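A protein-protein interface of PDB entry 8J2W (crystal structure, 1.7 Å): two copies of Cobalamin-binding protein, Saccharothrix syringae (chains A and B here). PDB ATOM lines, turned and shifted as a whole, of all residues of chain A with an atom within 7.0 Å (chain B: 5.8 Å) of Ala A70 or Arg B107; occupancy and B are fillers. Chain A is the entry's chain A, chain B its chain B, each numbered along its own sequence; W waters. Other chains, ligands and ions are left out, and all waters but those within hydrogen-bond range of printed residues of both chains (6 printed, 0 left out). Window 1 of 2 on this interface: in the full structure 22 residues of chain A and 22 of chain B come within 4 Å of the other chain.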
ATOM      1  N   LEU A  14      -4.747   7.334  11.983  1.00  0.00           N
ATOM      2  CA  LEU A  14      -3.993   8.285  11.183  1.00  0.00           C
ATOM      3  C   LEU A  14      -3.822   9.611  11.920  1.00  0.00           C
ATOM      4  O   LEU A  14      -2.732  10.175  11.915  1.00  0.00           O
ATOM      5  CB  LEU A  14      -4.658   8.523   9.806  1.00  0.00           C
ATOM      6  CG  LEU A  14      -4.687   7.307   8.873  1.00  0.00           C
ATOM      7  CD1 LEU A  14      -5.341   7.654   7.581  1.00  0.00           C
ATOM      8  CD2 LEU A  14      -3.281   6.760   8.653  1.00  0.00           C
ATOM      9  N   GLU A  19       1.007   3.901  13.589  1.00  0.00           N
ATOM     10  CA  GLU A  19       1.188   3.029  12.439  1.00  0.00           C
ATOM     11  C   GLU A  19       0.725   1.604  12.736  1.00  0.00           C
ATOM     12  O   GLU A  19       0.069   0.982  11.910  1.00  0.00           O
ATOM     13  CB  GLU A  19       2.639   2.990  12.037  1.00  0.00           C
ATOM     14  CG  GLU A  19       2.853   2.276  10.732  1.00  0.00           C
ATOM     15  CD  GLU A  19       4.310   2.115  10.365  1.00  0.00           C
ATOM     16  OE1 GLU A  19       5.090   3.086  10.515  1.00  0.00           O
ATOM     17  OE2 GLU A  19       4.666   1.009   9.902  1.00  0.00           O
ATOM     18  N   GLN A  48      -7.254   9.515   2.754  1.00  0.00           N
ATOM     19  CA  GLN A  48      -6.300  10.464   2.213  1.00  0.00           C
ATOM     20  C   GLN A  48      -6.970  11.694   1.606  1.00  0.00           C
ATOM     21  O   GLN A  48      -6.457  12.804   1.735  1.00  0.00           O
ATOM     22  CB  GLN A  48      -5.362   9.780   1.161  1.00  0.00           C
ATOM     23  CG  GLN A  48      -4.371   8.757   1.768  1.00  0.00           C
ATOM     24  CD  GLN A  48      -3.341   9.401   2.708  1.00  0.00           C
ATOM     25  OE1 GLN A  48      -3.277   9.100   3.915  1.00  0.00           O
ATOM     26  NE2 GLN A  48      -2.528  10.293   2.150  1.00  0.00           N
ATOM     27  N   GLU A  65      -0.527  15.703   8.354  1.00  0.00           N
ATOM     28  CA  GLU A  65      -0.682  15.015   7.078  1.00  0.00           C
ATOM     29  C   GLU A  65       0.463  14.043   6.789  1.00  0.00           C
ATOM     30  O   GLU A  65       0.204  12.878   6.475  1.00  0.00           O
ATOM     31  CB  GLU A  65      -0.882  15.985   5.904  1.00  0.00           C
ATOM     32  CG  GLU A  65      -0.761  15.299   4.541  1.00  0.00           C
ATOM     33  CD  GLU A  65       0.658  15.135   4.038  1.00  0.00           C
ATOM     34  OE1 GLU A  65       1.397  16.145   4.104  1.00  0.00           O
ATOM     35  OE2 GLU A  65       1.031  14.026   3.584  1.00  0.00           O
ATOM     36  N   HIS A  66       1.720  14.496   6.957  1.00  0.00           N
ATOM     37  CA  HIS A  66       2.877  13.650   6.700  1.00  0.00           C
ATOM     38  C   HIS A  66       2.820  12.371   7.539  1.00  0.00           C
ATOM     39  O   HIS A  66       3.137  11.295   7.034  1.00  0.00           O
ATOM     40  CB  HIS A  66       4.204  14.374   6.981  1.00  0.00           C
ATOM     41  CG  HIS A  66       4.703  15.216   5.851  1.00  0.00           C
ATOM     42  ND1 HIS A  66       6.035  15.508   5.591  1.00  0.00           N
ATOM     43  CD2 HIS A  66       3.986  15.896   4.942  1.00  0.00           C
ATOM     44  CE1 HIS A  66       6.097  16.322   4.525  1.00  0.00           C
ATOM     45  NE2 HIS A  66       4.859  16.584   4.124  1.00  0.00           N
ATOM     46  N   ALA A  67       2.456  12.493   8.822  1.00  0.00           N
ATOM     47  CA  ALA A  67       2.379  11.332   9.702  1.00  0.00           C
ATOM     48  C   ALA A  67       1.375  10.314   9.163  1.00  0.00           C
ATOM     49  O   ALA A  67       1.644   9.118   9.090  1.00  0.00           O
ATOM     50  CB  ALA A  67       1.956  11.749  11.108  1.00  0.00           C
ATOM     51  N   ALA A  68       0.220  10.829   8.757  1.00  0.00           N
ATOM     52  CA  ALA A  68      -0.868  10.005   8.255  1.00  0.00           C
ATOM     53  C   ALA A  68      -0.501   9.324   6.937  1.00  0.00           C
ATOM     54  O   ALA A  68      -0.676   8.130   6.776  1.00  0.00           O
ATOM     55  CB  ALA A  68      -2.094  10.872   8.085  1.00  0.00           C
ATOM     56  N   THR A  69       0.018  10.105   6.003  1.00  0.00           N
ATOM     57  CA  THR A  69       0.352   9.622   4.676  1.00  0.00           C
ATOM     58  C   THR A  69       1.375   8.496   4.744  1.00  0.00           C
ATOM     59  O   THR A  69       1.233   7.496   4.055  1.00  0.00           O
ATOM     60  CB  THR A  69       0.810  10.769   3.789  1.00  0.00           C
ATOM     61  OG1 THR A  69      -0.279  11.688   3.610  1.00  0.00           O
ATOM     62  CG2 THR A  69       1.316  10.284   2.462  1.00  0.00           C
ATOM     63  N   ALA A  70       2.389   8.646   5.602  1.00  0.00           N
ATOM     64  CA  ALA A  70       3.403   7.611   5.727  1.00  0.00           C
ATOM     65  C   ALA A  70       2.796   6.303   6.253  1.00  0.00           C
ATOM     66  O   ALA A  70       3.207   5.208   5.866  1.00  0.00           O
ATOM     67  CB  ALA A  70       4.536   8.083   6.618  1.00  0.00           C
ATOM     68  N   ILE A  71       1.802   6.415   7.145  1.00  0.00           N
ATOM     69  CA  ILE A  71       1.109   5.244   7.650  1.00  0.00           C
ATOM     70  C   ILE A  71       0.246   4.618   6.558  1.00  0.00           C
ATOM     71  O   ILE A  71       0.238   3.405   6.398  1.00  0.00           O
ATOM     72  CB  ILE A  71       0.271   5.609   8.917  1.00  0.00           C
ATOM     73  CG1 ILE A  71       1.212   6.031  10.067  1.00  0.00           C
ATOM     74  CG2 ILE A  71      -0.679   4.425   9.302  1.00  0.00           C
ATOM     75  CD1 ILE A  71       0.493   6.706  11.203  1.00  0.00           C
ATOM     76  N   SER A  72      -0.468   5.447   5.789  1.00  0.00           N
ATOM     77  CA  SER A  72      -1.238   4.936   4.667  1.00  0.00           C
ATOM     78  C   SER A  72      -0.349   4.162   3.684  1.00  0.00           C
ATOM     79  O   SER A  72      -0.747   3.112   3.194  1.00  0.00           O
ATOM     80  CB  SER A  72      -1.978   6.068   3.969  1.00  0.00           C
ATOM     81  OG  SER A  72      -3.042   6.557   4.761  1.00  0.00           O
ATOM     82  N   GLU A  73       0.880   4.643   3.444  1.00  0.00           N
ATOM     83  CA  GLU A  73       1.828   3.891   2.631  1.00  0.00           C
ATOM     84  C   GLU A  73       2.176   2.539   3.240  1.00  0.00           C
ATOM     85  O   GLU A  73       2.358   1.574   2.500  1.00  0.00           O
ATOM     86  CB  GLU A  73       3.105   4.701   2.359  1.00  0.00           C
ATOM     87  CG  GLU A  73       2.818   5.909   1.463  1.00  0.00           C
ATOM     88  CD  GLU A  73       3.984   6.486   0.665  1.00  0.00           C
ATOM     89  OE1 GLU A  73       5.063   6.685   1.269  1.00  0.00           O
ATOM     90  OE2 GLU A  73       3.808   6.785  -0.545  1.00  0.00           O
ATOM     91  N   ARG A  74       2.295   2.472   4.573  1.00  0.00           N
ATOM     92  CA  ARG A  74       2.600   1.218   5.253  1.00  0.00           C
ATOM     93  C   ARG A  74       1.403   0.270   5.168  1.00  0.00           C
ATOM     94  O   ARG A  74       1.585  -0.930   5.009  1.00  0.00           O
ATOM     95  CB  ARG A  74       3.029   1.457   6.711  1.00  0.00           C
ATOM     96  CG  ARG A  74       4.399   2.108   6.861  1.00  0.00           C
ATOM     97  CD  ARG A  74       5.529   1.203   6.299  1.00  0.00           C
ATOM     98  NE  ARG A  74       6.754   1.239   7.083  1.00  0.00           N
ATOM     99  CZ  ARG A  74       6.908   0.577   8.228  1.00  0.00           C
ATOM    100  NH1 ARG A  74       6.385  -0.628   8.414  1.00  0.00           N
ATOM    101  NH2 ARG A  74       7.581   1.146   9.211  1.00  0.00           N
ATOM    102  N   VAL A  75       0.178   0.816   5.248  1.00  0.00           N
ATOM    103  CA  VAL A  75      -1.026   0.016   5.085  1.00  0.00           C
ATOM    104  C   VAL A  75      -1.051  -0.582   3.679  1.00  0.00           C
ATOM    105  O   VAL A  75      -1.326  -1.777   3.518  1.00  0.00           O
ATOM    106  CB  VAL A  75      -2.326   0.819   5.377  1.00  0.00           C
ATOM    107  CG1 VAL A  75      -3.570   0.025   4.981  1.00  0.00           C
ATOM    108  CG2 VAL A  75      -2.398   1.221   6.850  1.00  0.00           C
ATOM    109  N   LEU A 104       1.390   8.120  -3.772  1.00  0.00           N
ATOM    110  CA  LEU A 104       0.456   7.181  -3.168  1.00  0.00           C
ATOM    111  C   LEU A 104      -0.685   6.777  -4.106  1.00  0.00           C
ATOM    112  O   LEU A 104      -1.006   5.576  -4.199  1.00  0.00           O
ATOM    113  CB  LEU A 104      -0.085   7.768  -1.849  1.00  0.00           C
ATOM    114  CG  LEU A 104      -0.702   6.810  -0.841  1.00  0.00           C
ATOM    115  CD1 LEU A 104      -0.653   7.404   0.551  1.00  0.00           C
ATOM    116  CD2 LEU A 104      -2.125   6.507  -1.145  1.00  0.00           C
ATOM    117  N   ILE B  76      12.445  -2.377   3.963  1.00  0.00           N
ATOM    118  CA  ILE B  76      12.474  -1.758   5.280  1.00  0.00           C
ATOM    119  C   ILE B  76      11.136  -1.943   6.005  1.00  0.00           C
ATOM    120  O   ILE B  76      11.136  -2.263   7.195  1.00  0.00           O
ATOM    121  CB  ILE B  76      12.907  -0.273   5.195  1.00  0.00           C
ATOM    122  CG1 ILE B  76      14.379  -0.122   4.776  1.00  0.00           C
ATOM    123  CG2 ILE B  76      12.670   0.439   6.533  1.00  0.00           C
ATOM    124  CD1 ILE B  76      14.716   1.246   4.205  1.00  0.00           C
ATOM    125  N   VAL B  94      10.506  11.559  14.149  1.00  0.00           N
ATOM    126  CA  VAL B  94      11.549  11.518  13.138  1.00  0.00           C
ATOM    127  C   VAL B  94      11.087  12.328  11.928  1.00  0.00           C
ATOM    128  O   VAL B  94      10.017  12.059  11.386  1.00  0.00           O
ATOM    129  CB  VAL B  94      11.888  10.070  12.738  1.00  0.00           C
ATOM    130  CG1 VAL B  94      12.849  10.055  11.539  1.00  0.00           C
ATOM    131  CG2 VAL B  94      12.470   9.290  13.906  1.00  0.00           C
ATOM    132  N   ALA B 103      14.081  10.516   2.437  1.00  0.00           N
ATOM    133  CA  ALA B 103      13.359   9.955   3.570  1.00  0.00           C
ATOM    134  C   ALA B 103      13.912   8.601   4.025  1.00  0.00           C
ATOM    135  O   ALA B 103      13.801   8.239   5.194  1.00  0.00           O
ATOM    136  CB  ALA B 103      11.869   9.838   3.211  1.00  0.00           C
ATOM    137  N   LEU B 104      14.547   7.844   3.121  1.00  0.00           N
ATOM    138  CA  LEU B 104      14.934   6.484   3.450  1.00  0.00           C
ATOM    139  C   LEU B 104      15.945   6.401   4.600  1.00  0.00           C
ATOM    140  O   LEU B 104      15.800   5.559   5.494  1.00  0.00           O
ATOM    141  CB  LEU B 104      15.485   5.776   2.192  1.00  0.00           C
ATOM    142  CG  LEU B 104      15.462   4.247   2.195  1.00  0.00           C
ATOM    143  CD1 LEU B 104      15.410   3.678   0.772  1.00  0.00           C
ATOM    144  CD2 LEU B 104      16.686   3.677   2.849  1.00  0.00           C
ATOM    145  N   PRO B 105      16.987   7.258   4.658  1.00  0.00           N
ATOM    146  CA  PRO B 105      17.892   7.236   5.811  1.00  0.00           C
ATOM    147  C   PRO B 105      17.126   7.428   7.121  1.00  0.00           C
ATOM    148  O   PRO B 105      17.420   6.776   8.128  1.00  0.00           O
ATOM    149  CB  PRO B 105      18.860   8.405   5.555  1.00  0.00           C
ATOM    150  CG  PRO B 105      18.729   8.769   4.166  1.00  0.00           C
ATOM    151  CD  PRO B 105      17.371   8.268   3.657  1.00  0.00           C
ATOM    152  N   ALA B 106      16.140   8.332   7.100  1.00  0.00           N
ATOM    153  CA  ALA B 106      15.338   8.615   8.286  1.00  0.00           C
ATOM    154  C   ALA B 106      14.431   7.433   8.639  1.00  0.00           C
ATOM    155  O   ALA B 106      14.194   7.165   9.820  1.00  0.00           O
ATOM    156  CB  ALA B 106      14.549   9.858   8.104  1.00  0.00           C
ATOM    157  N   ARG B 107      13.929   6.726   7.619  1.00  0.00           N
ATOM    158  CA  ARG B 107      13.112   5.545   7.855  1.00  0.00           C
ATOM    159  C   ARG B 107      13.932   4.455   8.542  1.00  0.00           C
ATOM    160  O   ARG B 107      13.411   3.767   9.417  1.00  0.00           O
ATOM    161  CB  ARG B 107      12.480   5.057   6.540  1.00  0.00           C
ATOM    162  CG  ARG B 107      11.594   3.807   6.704  1.00  0.00           C
ATOM    163  CD  ARG B 107      10.441   3.943   7.693  1.00  0.00           C
ATOM    164  NE  ARG B 107       9.166   4.364   7.111  1.00  0.00           N
ATOM    165  CZ  ARG B 107       8.038   4.523   7.810  1.00  0.00           C
ATOM    166  NH1 ARG B 107       7.965   4.212   9.094  1.00  0.00           N
ATOM    167  NH2 ARG B 107       6.954   4.983   7.198  1.00  0.00           N
ATOM    168  N   ILE B 108      15.209   4.287   8.145  1.00  0.00           N
ATOM    169  CA  ILE B 108      16.071   3.335   8.824  1.00  0.00           C
ATOM    170  C   ILE B 108      16.253   3.686  10.305  1.00  0.00           C
ATOM    171  O   ILE B 108      16.197   2.809  11.166  1.00  0.00           O
ATOM    172  CB  ILE B 108      17.424   3.196   8.095  1.00  0.00           C
ATOM    173  CG1 ILE B 108      17.221   2.583   6.691  1.00  0.00           C
ATOM    174  CG2 ILE B 108      18.404   2.380   8.903  1.00  0.00           C
ATOM    175  CD1 ILE B 108      18.465   2.646   5.803  1.00  0.00           C
ATOM    176  N   VAL B 109      16.499   4.965  10.591  1.00  0.00           N
ATOM    177  CA  VAL B 109      16.582   5.431  11.975  1.00  0.00           C
ATOM    178  C   VAL B 109      15.307   5.089  12.739  1.00  0.00           C
ATOM    179  O   VAL B 109      15.373   4.486  13.818  1.00  0.00           O
ATOM    180  CB  VAL B 109      16.892   6.947  12.064  1.00  0.00           C
ATOM    181  CG1 VAL B 109      16.814   7.433  13.526  1.00  0.00           C
ATOM    182  CG2 VAL B 109      18.231   7.262  11.450  1.00  0.00           C
ATOM    183  N   ALA B 110      14.144   5.414  12.152  1.00  0.00           N
ATOM    184  CA  ALA B 110      12.861   5.094  12.765  1.00  0.00           C
ATOM    185  C   ALA B 110      12.710   3.613  13.105  1.00  0.00           C
ATOM    186  O   ALA B 110      12.278   3.260  14.202  1.00  0.00           O
ATOM    187  CB  ALA B 110      11.710   5.520  11.876  1.00  0.00           C
ATOM    188  N   GLU B 111      13.067   2.737  12.157  1.00  0.00           N
ATOM    189  CA  GLU B 111      12.886   1.310  12.356  1.00  0.00           C
ATOM    190  C   GLU B 111      13.804   0.757  13.435  1.00  0.00           C
ATOM    191  O   GLU B 111      13.376  -0.075  14.244  1.00  0.00           O
ATOM    192  CB  GLU B 111      13.124   0.503  11.073  1.00  0.00           C
ATOM    193  CG  GLU B 111      12.029   0.687  10.079  1.00  0.00           C
ATOM    194  CD  GLU B 111      10.631   0.404  10.565  1.00  0.00           C
ATOM    195  OE1 GLU B 111      10.405  -0.411  11.496  1.00  0.00           O
ATOM    196  OE2 GLU B 111       9.736   1.042   9.988  1.00  0.00           O
ATOM    197  N   VAL B 112      15.060   1.215  13.421  1.00  0.00           N
ATOM    198  CA  VAL B 112      16.025   0.802  14.424  1.00  0.00           C
ATOM    199  C   VAL B 112      15.595   1.238  15.827  1.00  0.00           C
ATOM    200  O   VAL B 112      15.651   0.436  16.763  1.00  0.00           O
ATOM    201  CB  VAL B 112      17.458   1.267  14.056  1.00  0.00           C
ATOM    202  CG1 VAL B 112      18.420   1.056  15.228  1.00  0.00           C
ATOM    203  CG2 VAL B 112      17.961   0.538  12.797  1.00  0.00           C
ATOM    204  N   ARG B 114      12.445   1.820  16.802  1.00  0.00           N
ATOM    205  CA  ARG B 114      11.336   0.951  17.170  1.00  0.00           C
ATOM    206  C   ARG B 114      11.795  -0.423  17.663  1.00  0.00           C
ATOM    207  O   ARG B 114      11.201  -0.979  18.586  1.00  0.00           O
ATOM    208  CB  ARG B 114      10.367   0.741  16.002  1.00  0.00           C
ATOM    209  CG  ARG B 114       9.563   1.938  15.684  1.00  0.00           C
ATOM    210  CD  ARG B 114       8.649   1.701  14.518  1.00  0.00           C
ATOM    211  NE  ARG B 114       7.779   2.853  14.323  1.00  0.00           N
ATOM    212  CZ  ARG B 114       7.115   3.113  13.206  1.00  0.00           C
ATOM    213  NH1 ARG B 114       7.249   2.349  12.127  1.00  0.00           N
ATOM    214  NH2 ARG B 114       6.325   4.186  13.158  1.00  0.00           N
ATOM    215  N   PHE B 122       6.882   8.760  12.437  1.00  0.00           N
ATOM    216  CA  PHE B 122       7.700   9.089  11.288  1.00  0.00           C
ATOM    217  C   PHE B 122       7.003  10.110  10.391  1.00  0.00           C
ATOM    218  O   PHE B 122       5.920   9.836   9.870  1.00  0.00           O
ATOM    219  CB  PHE B 122       7.974   7.829  10.481  1.00  0.00           C
ATOM    220  CG  PHE B 122       8.860   8.062   9.286  1.00  0.00           C
ATOM    221  CD1 PHE B 122      10.221   8.296   9.440  1.00  0.00           C
ATOM    222  CD2 PHE B 122       8.338   8.056   8.005  1.00  0.00           C
ATOM    223  CE1 PHE B 122      11.032   8.511   8.327  1.00  0.00           C
ATOM    224  CE2 PHE B 122       9.164   8.234   6.900  1.00  0.00           C
ATOM    225  CZ  PHE B 122      10.501   8.471   7.067  1.00  0.00           C
ATOM    226  N   LEU B 123       7.644  11.269  10.215  1.00  0.00           N
ATOM    227  CA  LEU B 123       7.091  12.321   9.384  1.00  0.00           C
ATOM    228  C   LEU B 123       7.743  12.331   8.003  1.00  0.00           C
ATOM    229  O   LEU B 123       7.138  12.830   7.062  1.00  0.00           O
ATOM    230  CB  LEU B 123       7.277  13.683  10.031  1.00  0.00           C
ATOM    231  CG  LEU B 123       6.674  13.857  11.402  1.00  0.00           C
ATOM    232  CD1 LEU B 123       6.798  15.301  11.862  1.00  0.00           C
ATOM    233  CD2 LEU B 123       5.241  13.376  11.451  1.00  0.00           C
HETATM  234  O   HOH W   1       3.372   5.575  14.210  1.00  0.00           O
HETATM  235  O   HOH W   2       7.764  -0.739  11.921  1.00  0.00           O
HETATM  236  O   HOH W   3       4.044   8.080  10.137  1.00  0.00           O
HETATM  237  O   HOH W   4       4.792   5.391   8.939  1.00  0.00           O
HETATM  238  O   HOH W   5       6.792  12.334   4.355  1.00  0.00           O
HETATM  239  O   HOH W   6       5.630   4.945   4.927  1.00  0.00           O
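NH1 of Arg B107 lies within salt-bridge range of OE1 of Glu A19.
The side-chain carboxylate of Glu A19 is in salt-bridge range of the guanidinium group of Arg B114, at 2.8 Å.
The backbone carbonyl oxygen (O) of Leu B123 is in hydrogen-bond range of a ring nitrogen (ND1) of His A66.
NH2 of Arg A74 is in salt-bridge range of OE1 of Glu B111 (3.95 Å).
NH2 of Arg A74 sits close to NH1 of Arg B107, 3.1 Å away.
The guanidinium group (NH1) of Arg B114 lies close to the guanidinium group (NH2) of Arg A74.
The side-chain carboxylate (OE2) of Glu B111 lies within salt-bridge range of the guanidinium group (NH1) of Arg B114 (3.5 Å).
NH1 of Arg A74 lies within salt-bridge range of OE2 of Glu A19, at 2.8 Å.
The side-chain carboxylate of Glu A65 lies close to a ring nitrogen (NE2) of His A66 (3.5 Å).
N of Leu B123 is in hydrogen-bond range of O of Val B94 (2.8 Å).
The side-chain carboxylate (OE2) of Glu B111 lies within salt-bridge range of the guanidinium group (NH1) of Arg B107.
Among the printed residues, pairs that only touch across the chains: Ala A67 with Leu B123, Ala A67 with Phe B122, Ala A70 with Phe B122 and Ala A70 with Arg B107.
Ala A70 touches just these residues of chain B: Arg B107 and Phe B122.
Printed residues of chain A within 4 Å of Arg B107: Glu A19 (3.4 Å), Ala A70 (3.97 Å) and Arg A74 (3.1 Å).
Of the printed residues of chain A, Phe B122 touches Ala A67 (3.8 Å) and Ala A70 (3.9 Å).
Of the printed residues of chain A, Glu B111 touches Arg A74 (2.3 Å).
Glu A65 touches none of the printed residues of chain B.
Val A75 touches none of the printed residues of chain B.
Of the 15 printed residues of chain A, 5 touch a printed residue of chain B.
Hydrophobic or aromatic side chains of chain A within 4 Å of the printed part of chain B: His A66, Ala A67 and Ala A70.
Of the 15 printed residues of chain B, 5 touch a printed residue of chain A.
Along chain B the printed residues that touch a printed residue of chain A span positions 107 to 123.
Position printed for both chains: 104.
Of the 10 pairs that touch across the chains among the printed residues, none has its exchanged pair printed and touching as well.
Water W3 lies within hydrogen-bond range of the backbone carbonyl oxygen (O) of Phe B122 (2.6 Å) and the backbone carbonyl oxygen (O) of Ala A67 (2.8 Å).
Water W6 lies within hydrogen-bond range of O of Ala A70 (2.6 Å) and NH2 of Arg B107 (2.6 Å).
Water W2 lies within hydrogen-bond range of the side-chain carboxylate (OE1) of Glu B111 (2.7 Å), the guanidinium group (NH1) of Arg B114 (3.1 Å) and the guanidinium group (NH2) of Arg A74 (3.3 Å).
Water W5 lies within hydrogen-bond range of O of Leu B123 (2.8 Å) and ND1 of His A66 (3.5 Å).
Water W4 lies within hydrogen-bond range of the guanidinium group of Arg B107 (2.8 Å), the side-chain carboxylate of Glu A19 (2.8 Å) and the backbone carbonyl oxygen of Ala A70 (3.5 Å).
Water W1 bridges the backbone NH of Glu A19 (3.0 Å) and the guanidinium group of Arg B114 (3.4 Å).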
